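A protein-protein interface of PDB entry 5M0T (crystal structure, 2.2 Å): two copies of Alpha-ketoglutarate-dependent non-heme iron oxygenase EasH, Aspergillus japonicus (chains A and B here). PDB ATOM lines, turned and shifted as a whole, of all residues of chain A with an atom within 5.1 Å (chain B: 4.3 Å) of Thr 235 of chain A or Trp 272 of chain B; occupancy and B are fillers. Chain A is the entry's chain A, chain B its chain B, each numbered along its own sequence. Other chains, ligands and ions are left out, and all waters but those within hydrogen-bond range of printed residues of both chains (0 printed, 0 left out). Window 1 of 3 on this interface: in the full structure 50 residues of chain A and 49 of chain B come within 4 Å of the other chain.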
ATOM      1  N   THR A 115     -30.266  29.717 -26.116  1.00  0.00           N
ATOM      2  CA  THR A 115     -28.948  29.106 -26.306  1.00  0.00           C
ATOM      3  C   THR A 115     -27.958  29.621 -25.240  1.00  0.00           C
ATOM      4  O   THR A 115     -27.257  28.822 -24.603  1.00  0.00           O
ATOM      5  CB  THR A 115     -28.413  29.214 -27.747  1.00  0.00           C
ATOM      6  OG1 THR A 115     -27.132  28.582 -27.820  1.00  0.00           O
ATOM      7  CG2 THR A 115     -28.274  30.646 -28.230  1.00  0.00           C
ATOM      8  N   GLN A 230     -32.521  30.890 -30.013  1.00  0.00           N
ATOM      9  CA  GLN A 230     -32.019  30.071 -31.096  1.00  0.00           C
ATOM     10  C   GLN A 230     -33.054  29.080 -31.603  1.00  0.00           C
ATOM     11  O   GLN A 230     -33.873  28.584 -30.840  1.00  0.00           O
ATOM     12  CB  GLN A 230     -30.786  29.342 -30.571  1.00  0.00           C
ATOM     13  CG  GLN A 230     -30.179  28.267 -31.445  1.00  0.00           C
ATOM     14  CD  GLN A 230     -28.795  27.894 -30.936  1.00  0.00           C
ATOM     15  OE1 GLN A 230     -27.887  28.720 -30.923  1.00  0.00           O
ATOM     16  NE2 GLN A 230     -28.653  26.675 -30.463  1.00  0.00           N
ATOM     17  N   GLN A 233     -33.639  23.274 -33.514  1.00  0.00           N
ATOM     18  CA  GLN A 233     -32.825  22.219 -34.149  1.00  0.00           C
ATOM     19  C   GLN A 233     -31.326  22.280 -33.764  1.00  0.00           C
ATOM     20  O   GLN A 233     -30.627  21.283 -33.926  1.00  0.00           O
ATOM     21  CB  GLN A 233     -32.962  22.237 -35.673  1.00  0.00           C
ATOM     22  CG  GLN A 233     -32.233  23.388 -36.359  1.00  0.00           C
ATOM     23  CD  GLN A 233     -32.613  23.536 -37.832  1.00  0.00           C
ATOM     24  OE1 GLN A 233     -32.588  22.569 -38.592  1.00  0.00           O
ATOM     25  NE2 GLN A 233     -32.957  24.756 -38.243  1.00  0.00           N
ATOM     26  N   PHE A 234     -30.856  23.437 -33.283  1.00  0.00           N
ATOM     27  CA  PHE A 234     -29.456  23.609 -32.853  1.00  0.00           C
ATOM     28  C   PHE A 234     -29.272  23.514 -31.337  1.00  0.00           C
ATOM     29  O   PHE A 234     -30.014  24.132 -30.548  1.00  0.00           O
ATOM     30  CB  PHE A 234     -28.872  24.932 -33.354  1.00  0.00           C
ATOM     31  CG  PHE A 234     -28.907  25.069 -34.841  1.00  0.00           C
ATOM     32  CD1 PHE A 234     -28.155  24.226 -35.640  1.00  0.00           C
ATOM     33  CD2 PHE A 234     -29.739  26.020 -35.456  1.00  0.00           C
ATOM     34  CE1 PHE A 234     -28.195  24.344 -37.028  1.00  0.00           C
ATOM     35  CE2 PHE A 234     -29.789  26.133 -36.838  1.00  0.00           C
ATOM     36  CZ  PHE A 234     -29.011  25.298 -37.628  1.00  0.00           C
ATOM     37  N   THR A 235     -28.258  22.742 -30.948  1.00  0.00           N
ATOM     38  CA  THR A 235     -27.904  22.526 -29.561  1.00  0.00           C
ATOM     39  C   THR A 235     -27.612  23.862 -28.863  1.00  0.00           C
ATOM     40  O   THR A 235     -26.880  24.691 -29.391  1.00  0.00           O
ATOM     41  CB  THR A 235     -26.673  21.597 -29.456  1.00  0.00           C
ATOM     42  OG1 THR A 235     -26.925  20.372 -30.173  1.00  0.00           O
ATOM     43  CG2 THR A 235     -26.354  21.273 -28.006  1.00  0.00           C
ATOM     44  N   PRO A 236     -28.204  24.085 -27.680  1.00  0.00           N
ATOM     45  CA  PRO A 236     -27.867  25.264 -26.893  1.00  0.00           C
ATOM     46  C   PRO A 236     -26.405  25.329 -26.408  1.00  0.00           C
ATOM     47  O   PRO A 236     -25.802  24.300 -26.082  1.00  0.00           O
ATOM     48  CB  PRO A 236     -28.797  25.144 -25.680  1.00  0.00           C
ATOM     49  CG  PRO A 236     -29.958  24.357 -26.167  1.00  0.00           C
ATOM     50  CD  PRO A 236     -29.366  23.369 -27.123  1.00  0.00           C
ATOM     51  N   VAL A 237     -25.858  26.533 -26.341  1.00  0.00           N
ATOM     52  CA  VAL A 237     -24.545  26.742 -25.742  1.00  0.00           C
ATOM     53  C   VAL A 237     -24.564  26.420 -24.234  1.00  0.00           C
ATOM     54  O   VAL A 237     -23.596  25.856 -23.713  1.00  0.00           O
ATOM     55  CB  VAL A 237     -24.033  28.171 -26.011  1.00  0.00           C
ATOM     56  CG1 VAL A 237     -22.793  28.479 -25.185  1.00  0.00           C
ATOM     57  CG2 VAL A 237     -23.733  28.348 -27.494  1.00  0.00           C
ATOM     58  N   GLU A 238     -25.664  26.760 -23.557  1.00  0.00           N
ATOM     59  CA  GLU A 238     -25.832  26.497 -22.125  1.00  0.00           C
ATOM     60  C   GLU A 238     -26.669  25.258 -21.868  1.00  0.00           C
ATOM     61  O   GLU A 238     -27.788  25.156 -22.368  1.00  0.00           O
ATOM     62  CB  GLU A 238     -26.486  27.688 -21.454  1.00  0.00           C
ATOM     63  CG  GLU A 238     -25.584  28.914 -21.414  1.00  0.00           C
ATOM     64  CD  GLU A 238     -26.284  30.140 -20.875  1.00  0.00           C
ATOM     65  OE1 GLU A 238     -27.433  30.025 -20.370  1.00  0.00           O
ATOM     66  OE2 GLU A 238     -25.688  31.238 -20.977  1.00  0.00           O
ATOM     67  N   ALA A 239     -26.123  24.330 -21.081  1.00  0.00           N
ATOM     68  CA  ALA A 239     -26.751  23.034 -20.831  1.00  0.00           C
ATOM     69  C   ALA A 239     -27.897  23.137 -19.842  1.00  0.00           C
ATOM     70  O   ALA A 239     -27.758  23.735 -18.787  1.00  0.00           O
ATOM     71  CB  ALA A 239     -25.726  22.028 -20.321  1.00  0.00           C
ATOM     72  N   SER A 240     -29.021  22.532 -20.194  1.00  0.00           N
ATOM     73  CA  SER A 240     -30.210  22.524 -19.339  1.00  0.00           C
ATOM     74  C   SER A 240     -30.096  21.538 -18.170  1.00  0.00           C
ATOM     75  O   SER A 240     -30.799  21.694 -17.171  1.00  0.00           O
ATOM     76  CB  SER A 240     -31.453  22.223 -20.172  1.00  0.00           C
ATOM     77  OG  SER A 240     -31.337  20.974 -20.818  1.00  0.00           O
ATOM     78  N   VAL A 241     -29.204  20.547 -18.279  1.00  0.00           N
ATOM     79  CA  VAL A 241     -28.910  19.640 -17.155  1.00  0.00           C
ATOM     80  C   VAL A 241     -28.244  20.309 -15.944  1.00  0.00           C
ATOM     81  O   VAL A 241     -28.181  19.693 -14.899  1.00  0.00           O
ATOM     82  CB  VAL A 241     -28.027  18.430 -17.550  1.00  0.00           C
ATOM     83  CG1 VAL A 241     -28.698  17.594 -18.621  1.00  0.00           C
ATOM     84  CG2 VAL A 241     -26.625  18.866 -17.977  1.00  0.00           C
ATOM     85  N   TRP A 272     -36.046  16.499 -28.293  1.00  0.00           N
ATOM     86  CA  TRP A 272     -35.879  16.650 -26.848  1.00  0.00           C
ATOM     87  C   TRP A 272     -37.064  15.977 -26.122  1.00  0.00           C
ATOM     88  O   TRP A 272     -37.829  16.600 -25.393  1.00  0.00           O
ATOM     89  CB  TRP A 272     -35.712  18.124 -26.473  1.00  0.00           C
ATOM     90  CG  TRP A 272     -34.855  18.367 -25.283  1.00  0.00           C
ATOM     91  CD1 TRP A 272     -35.223  18.960 -24.113  1.00  0.00           C
ATOM     92  CD2 TRP A 272     -33.455  18.060 -25.156  1.00  0.00           C
ATOM     93  NE1 TRP A 272     -34.141  19.037 -23.259  1.00  0.00           N
ATOM     94  CE2 TRP A 272     -33.043  18.502 -23.882  1.00  0.00           C
ATOM     95  CE3 TRP A 272     -32.506  17.481 -26.009  1.00  0.00           C
ATOM     96  CZ2 TRP A 272     -31.736  18.339 -23.421  1.00  0.00           C
ATOM     97  CZ3 TRP A 272     -31.201  17.335 -25.551  1.00  0.00           C
ATOM     98  CH2 TRP A 272     -30.830  17.766 -24.270  1.00  0.00           C
ATOM     99  N   TRP B 113     -22.678  12.999 -30.715  1.00  0.00           N
ATOM    100  CA  TRP B 113     -23.322  12.360 -29.565  1.00  0.00           C
ATOM    101  C   TRP B 113     -24.590  11.615 -29.990  1.00  0.00           C
ATOM    102  O   TRP B 113     -24.979  11.652 -31.159  1.00  0.00           O
ATOM    103  CB  TRP B 113     -23.603  13.385 -28.451  1.00  0.00           C
ATOM    104  CG  TRP B 113     -24.434  14.605 -28.817  1.00  0.00           C
ATOM    105  CD1 TRP B 113     -25.115  14.856 -29.990  1.00  0.00           C
ATOM    106  CD2 TRP B 113     -24.730  15.697 -27.950  1.00  0.00           C
ATOM    107  NE1 TRP B 113     -25.763  16.061 -29.910  1.00  0.00           N
ATOM    108  CE2 TRP B 113     -25.543  16.600 -28.668  1.00  0.00           C
ATOM    109  CE3 TRP B 113     -24.356  16.019 -26.636  1.00  0.00           C
ATOM    110  CZ2 TRP B 113     -26.001  17.794 -28.109  1.00  0.00           C
ATOM    111  CZ3 TRP B 113     -24.806  17.214 -26.083  1.00  0.00           C
ATOM    112  CH2 TRP B 113     -25.626  18.084 -26.814  1.00  0.00           C
ATOM    113  N   CYS B 232     -22.776  17.060 -33.117  1.00  0.00           N
ATOM    114  CA  CYS B 232     -23.107  17.717 -31.851  1.00  0.00           C
ATOM    115  C   CYS B 232     -23.821  19.074 -31.976  1.00  0.00           C
ATOM    116  O   CYS B 232     -24.487  19.501 -31.027  1.00  0.00           O
ATOM    117  CB  CYS B 232     -21.870  17.872 -30.969  1.00  0.00           C
ATOM    118  SG  CYS B 232     -20.657  19.055 -31.606  1.00  0.00           S
ATOM    119  N   GLN B 233     -23.679  19.745 -33.125  1.00  0.00           N
ATOM    120  CA  GLN B 233     -24.370  21.020 -33.380  1.00  0.00           C
ATOM    121  C   GLN B 233     -25.903  20.884 -33.453  1.00  0.00           C
ATOM    122  O   GLN B 233     -26.593  21.886 -33.290  1.00  0.00           O
ATOM    123  CB  GLN B 233     -23.850  21.694 -34.644  1.00  0.00           C
ATOM    124  CG  GLN B 233     -24.306  21.043 -35.944  1.00  0.00           C
ATOM    125  CD  GLN B 233     -23.567  21.562 -37.167  1.00  0.00           C
ATOM    126  OE1 GLN B 233     -23.512  22.762 -37.399  1.00  0.00           O
ATOM    127  NE2 GLN B 233     -23.034  20.647 -37.980  1.00  0.00           N
ATOM    128  N   PHE B 234     -26.409  19.663 -33.699  1.00  0.00           N
ATOM    129  CA  PHE B 234     -27.844  19.394 -33.773  1.00  0.00           C
ATOM    130  C   PHE B 234     -28.421  18.783 -32.487  1.00  0.00           C
ATOM    131  O   PHE B 234     -27.867  17.831 -31.907  1.00  0.00           O
ATOM    132  CB  PHE B 234     -28.174  18.486 -34.956  1.00  0.00           C
ATOM    133  CG  PHE B 234     -27.766  19.057 -36.277  1.00  0.00           C
ATOM    134  CD1 PHE B 234     -28.351  20.221 -36.758  1.00  0.00           C
ATOM    135  CD2 PHE B 234     -26.756  18.454 -37.030  1.00  0.00           C
ATOM    136  CE1 PHE B 234     -27.961  20.759 -37.979  1.00  0.00           C
ATOM    137  CE2 PHE B 234     -26.360  18.992 -38.254  1.00  0.00           C
ATOM    138  CZ  PHE B 234     -26.965  20.147 -38.728  1.00  0.00           C
ATOM    139  N   THR B 235     -29.550  19.349 -32.066  1.00  0.00           N
ATOM    140  CA  THR B 235     -30.252  18.930 -30.864  1.00  0.00           C
ATOM    141  C   THR B 235     -30.629  17.440 -30.949  1.00  0.00           C
ATOM    142  O   THR B 235     -31.147  16.985 -31.965  1.00  0.00           O
ATOM    143  CB  THR B 235     -31.513  19.783 -30.650  1.00  0.00           C
ATOM    144  OG1 THR B 235     -31.156  21.174 -30.623  1.00  0.00           O
ATOM    145  CG2 THR B 235     -32.209  19.417 -29.341  1.00  0.00           C
ATOM    146  N   SER B 240     -31.492  14.598 -22.625  1.00  0.00           N
ATOM    147  CA  SER B 240     -30.570  14.145 -21.579  1.00  0.00           C
ATOM    148  C   SER B 240     -31.059  14.523 -20.170  1.00  0.00           C
ATOM    149  O   SER B 240     -30.631  13.907 -19.196  1.00  0.00           O
ATOM    150  CB  SER B 240     -29.179  14.698 -21.844  1.00  0.00           C
ATOM    151  OG  SER B 240     -29.197  16.105 -21.848  1.00  0.00           O
ATOM    152  N   GLY B 260     -25.321  13.238 -23.428  1.00  0.00           N
ATOM    153  CA  GLY B 260     -25.704  14.625 -23.208  1.00  0.00           C
ATOM    154  C   GLY B 260     -25.458  15.220 -21.840  1.00  0.00           C
ATOM    155  O   GLY B 260     -26.169  16.139 -21.437  1.00  0.00           O
ATOM    156  N   ARG B 262     -21.975  16.066 -20.925  1.00  0.00           N
ATOM    157  CA  ARG B 262     -20.690  16.796 -20.990  1.00  0.00           C
ATOM    158  C   ARG B 262     -20.655  17.762 -22.156  1.00  0.00           C
ATOM    159  O   ARG B 262     -21.473  17.688 -23.086  1.00  0.00           O
ATOM    160  CB  ARG B 262     -19.499  15.834 -21.085  1.00  0.00           C
ATOM    161  CG  ARG B 262     -19.037  15.301 -19.738  1.00  0.00           C
ATOM    162  CD  ARG B 262     -18.189  14.041 -19.879  1.00  0.00           C
ATOM    163  NE  ARG B 262     -17.958  13.426 -18.579  1.00  0.00           N
ATOM    164  CZ  ARG B 262     -17.034  13.808 -17.694  1.00  0.00           C
ATOM    165  NH1 ARG B 262     -16.199  14.825 -17.923  1.00  0.00           N
ATOM    166  NH2 ARG B 262     -16.954  13.158 -16.552  1.00  0.00           N
ATOM    167  N   THR B 263     -19.687  18.667 -22.085  1.00  0.00           N
ATOM    168  CA  THR B 263     -19.474  19.669 -23.097  1.00  0.00           C
ATOM    169  C   THR B 263     -18.932  19.000 -24.359  1.00  0.00           C
ATOM    170  O   THR B 263     -18.136  18.067 -24.286  1.00  0.00           O
ATOM    171  CB  THR B 263     -18.533  20.758 -22.564  1.00  0.00           C
ATOM    172  OG1 THR B 263     -19.213  21.486 -21.533  1.00  0.00           O
ATOM    173  CG2 THR B 263     -18.062  21.733 -23.659  1.00  0.00           C
ATOM    174  N   ILE B 271     -19.967  23.925 -26.767  1.00  0.00           N
ATOM    175  CA  ILE B 271     -21.395  24.051 -26.511  1.00  0.00           C
ATOM    176  C   ILE B 271     -21.846  22.993 -25.509  1.00  0.00           C
ATOM    177  O   ILE B 271     -21.123  22.022 -25.247  1.00  0.00           O
ATOM    178  CB  ILE B 271     -22.224  24.007 -27.822  1.00  0.00           C
ATOM    179  CG1 ILE B 271     -22.115  22.662 -28.534  1.00  0.00           C
ATOM    180  CG2 ILE B 271     -21.783  25.128 -28.769  1.00  0.00           C
ATOM    181  CD1 ILE B 271     -22.948  22.604 -29.800  1.00  0.00           C
ATOM    182  N   TRP B 272     -23.047  23.197 -24.956  1.00  0.00           N
ATOM    183  CA  TRP B 272     -23.552  22.413 -23.828  1.00  0.00           C
ATOM    184  C   TRP B 272     -22.627  22.609 -22.607  1.00  0.00           C
ATOM    185  O   TRP B 272     -22.024  21.683 -22.091  1.00  0.00           O
ATOM    186  CB  TRP B 272     -23.728  20.943 -24.232  1.00  0.00           C
ATOM    187  CG  TRP B 272     -24.837  20.242 -23.523  1.00  0.00           C
ATOM    188  CD1 TRP B 272     -24.726  19.157 -22.714  1.00  0.00           C
ATOM    189  CD2 TRP B 272     -26.243  20.557 -23.580  1.00  0.00           C
ATOM    190  NE1 TRP B 272     -25.966  18.782 -22.244  1.00  0.00           N
ATOM    191  CE2 TRP B 272     -26.910  19.639 -22.745  1.00  0.00           C
ATOM    192  CE3 TRP B 272     -26.991  21.554 -24.217  1.00  0.00           C
ATOM    193  CZ2 TRP B 272     -28.290  19.665 -22.548  1.00  0.00           C
ATOM    194  CZ3 TRP B 272     -28.371  21.584 -24.014  1.00  0.00           C
ATOM    195  CH2 TRP B 272     -29.003  20.637 -23.197  1.00  0.00           C
ATOM    196  N   THR B 273     -22.562  23.852 -22.166  1.00  0.00           N
ATOM    197  CA  THR B 273     -21.660  24.297 -21.133  1.00  0.00           C
ATOM    198  C   THR B 273     -22.400  24.702 -19.858  1.00  0.00           C
ATOM    199  O   THR B 273     -23.629  24.866 -19.860  1.00  0.00           O
ATOM    200  CB  THR B 273     -20.899  25.526 -21.651  1.00  0.00           C
ATOM    201  OG1 THR B 273     -21.824  26.592 -21.855  1.00  0.00           O
ATOM    202  CG2 THR B 273     -20.202  25.193 -22.972  1.00  0.00           C
ATOM    203  N   LEU B 279     -18.782  21.697 -18.653  1.00  0.00           N
ATOM    204  CA  LEU B 279     -20.010  21.339 -17.916  1.00  0.00           C
ATOM    205  C   LEU B 279     -19.710  20.447 -16.713  1.00  0.00           C
ATOM    206  O   LEU B 279     -20.184  20.715 -15.605  1.00  0.00           O
ATOM    207  CB  LEU B 279     -21.006  20.624 -18.839  1.00  0.00           C
ATOM    208  CG  LEU B 279     -22.289  20.042 -18.231  1.00  0.00           C
ATOM    209  CD1 LEU B 279     -23.070  21.121 -17.508  1.00  0.00           C
ATOM    210  CD2 LEU B 279     -23.163  19.391 -19.287  1.00  0.00           C
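The backbone NH of Thr 235 of chain A is in hydrogen-bond range of the backbone carbonyl oxygen of Gln 233 of chain B, at 3.0 Å.
OG1 of Thr 235 of chain A lies within hydrogen-bond range of O of Cys 232 of chain B, at 2.7 Å.
N of Thr 235 of chain A is in hydrogen-bond range of OG1 of Thr 235 of chain B, 3.3 Å away.
OG1 of Thr 235 of chain B lies close to O of Phe 234 of chain A (3.2 Å).
The backbone carbonyl oxygen of Gln 233 of chain A lies within hydrogen-bond range of the backbone NH of Thr 235 of chain B, 2.9 Å away.
The backbone carbonyl oxygen (O) of Val 237 of chain A sits at hydrogen-bond distance from the side-chain hydroxyl (OG1) of Thr 273 of chain B, 2.7 Å away.
The backbone carbonyl oxygen (O) of Val 237 of chain A sits at hydrogen-bond distance from the backbone NH (N) of Trp 272 of chain B (3.0 Å).
N of Ala 239 of chain A lies within hydrogen-bond range of O of Thr 273 of chain B (2.8 Å).
The backbone carbonyl oxygen (O) of Phe 234 of chain B lies close to the side-chain hydroxyl (OG1) of Thr 235 of chain A (3.2 Å).
The backbone carbonyl oxygen of Pro 236 of chain A lies within hydrogen-bond range of the backbone NH of Trp 272 of chain B, at 3.2 Å.
O of Thr 115 of chain A is in hydrogen-bond range of N of Glu 238 of chain A (2.8 Å).
The side-chain hydroxyl (OG1) of Thr 115 of chain A lies within hydrogen-bond range of the backbone NH (N) of Val 237 of chain A (2.8 Å).
The indole nitrogen (NE1) of Trp 113 of chain B sits at hydrogen-bond distance from the backbone carbonyl oxygen (O) of Phe 234 of chain B (3.4 Å).
The side-chain hydroxyl (OG1) of Thr 263 of chain B lies within hydrogen-bond range of the backbone NH (N) of Leu 279 of chain B, 2.9 Å away.
NE2 of Gln 230 of chain A lies within hydrogen-bond range of O of Phe 234 of chain A (2.9 Å).
O of Trp 272 of chain B is in hydrogen-bond range of OG1 of Thr 263 of chain B, 2.9 Å away.
Among the printed residues, pairs that only touch across the chains: Ser 240 of chain A with Trp 272 of chain B (3.3 Å), Trp 272 of chain A with Ser 240 of chain B (3.4 Å), Gln 233 of chain A with Phe 234 of chain B (3.4 Å), Phe 234 of chain A with Gln 233 of chain B (3.4 Å), Thr 235 of chain A with Trp 113 of chain B (3.4 Å), Glu 238 of chain A with Thr 273 of chain B (3.6 Å), Trp 272 of chain A with Trp 272 of chain B (3.6 Å), Val 241 of chain A with Ser 240 of chain B (3.6 Å), Ala 239 of chain A with Trp 272 of chain B (3.6 Å), Phe 234 of chain A with Phe 234 of chain B (3.7 Å), Val 241 of chain A with Leu 279 of chain B (3.7 Å), Val 237 of chain A with Ile 271 of chain B (3.8 Å), Ala 239 of chain A with Leu 279 of chain B (3.8 Å), Thr 235 of chain A with Trp 272 of chain B (3.9 Å), Trp 272 of chain A with Thr 235 of chain B (3.9 Å), Thr 235 of chain A with Ile 271 of chain B (3.9 Å), Glu 238 of chain A with Trp 272 of chain B (3.98 Å) and Pro 236 of chain A with Ile 271 of chain B (3.99 Å).
Of the printed residues of chain B, Thr 235 of chain A touches Trp 113 (3.4 Å), Cys 232 (2.7 Å), Gln 233 (3.0 Å), Phe 234 (3.2 Å), Thr 235 (3.3 Å), Ile 271 (3.9 Å) and Trp 272 (3.9 Å).
Trp 272 of chain B touches seven residues of chain A.
Of the printed residues of chain B, Glu 238 of chain A touches Trp 272 and Thr 273.
Of the printed residues of chain A, Trp 113 of chain B touches Thr 235 (3.4 Å).
Printed residues of chain A within 4 Å of Cys 232 of chain B: Thr 235 (2.7 Å).
Gly 260 of chain B touches none of the printed residues of chain A.
Gln 230 of chain A touches none of the printed residues of chain B.
The nearest residue of chain A that does not touch Trp 272 of chain B is Val 241 of chain A (4.3 Å).
Of the 12 printed residues of chain A, 10 touch a printed residue of chain B.
Hydrophobic or aromatic side chains of chain A that line the printed part of chain B: Phe 234, Pro 236, Val 237, Ala 239, Val 241 and Trp 272.
Among the printed residues, no Asp or Glu carboxylate lies within 4 Å of a Lys or Arg side-chain nitrogen of the other chain.
Phe 234 of chain A touches its own counterpart, Phe 234 of chain B.
Phe 234 of chain A touches Thr 235 of chain B, and with the chains exchanged Thr 235 of chain A touches Phe 234 of chain B.
Thr 235 of chain A touches Trp 272 of chain B, and with the chains exchanged Trp 272 of chain A touches Thr 235 of chain B.
Ser 240 of chain A touches Trp 272 of chain B, and with the chains exchanged Trp 272 of chain A touches Ser 240 of chain B.
Positions printed for both chains: 233, 234, 235, 240 and 272.
Of the 28 pairs that touch across the chains among the printed residues, 13 have their exchanged pair printed and touching as well.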
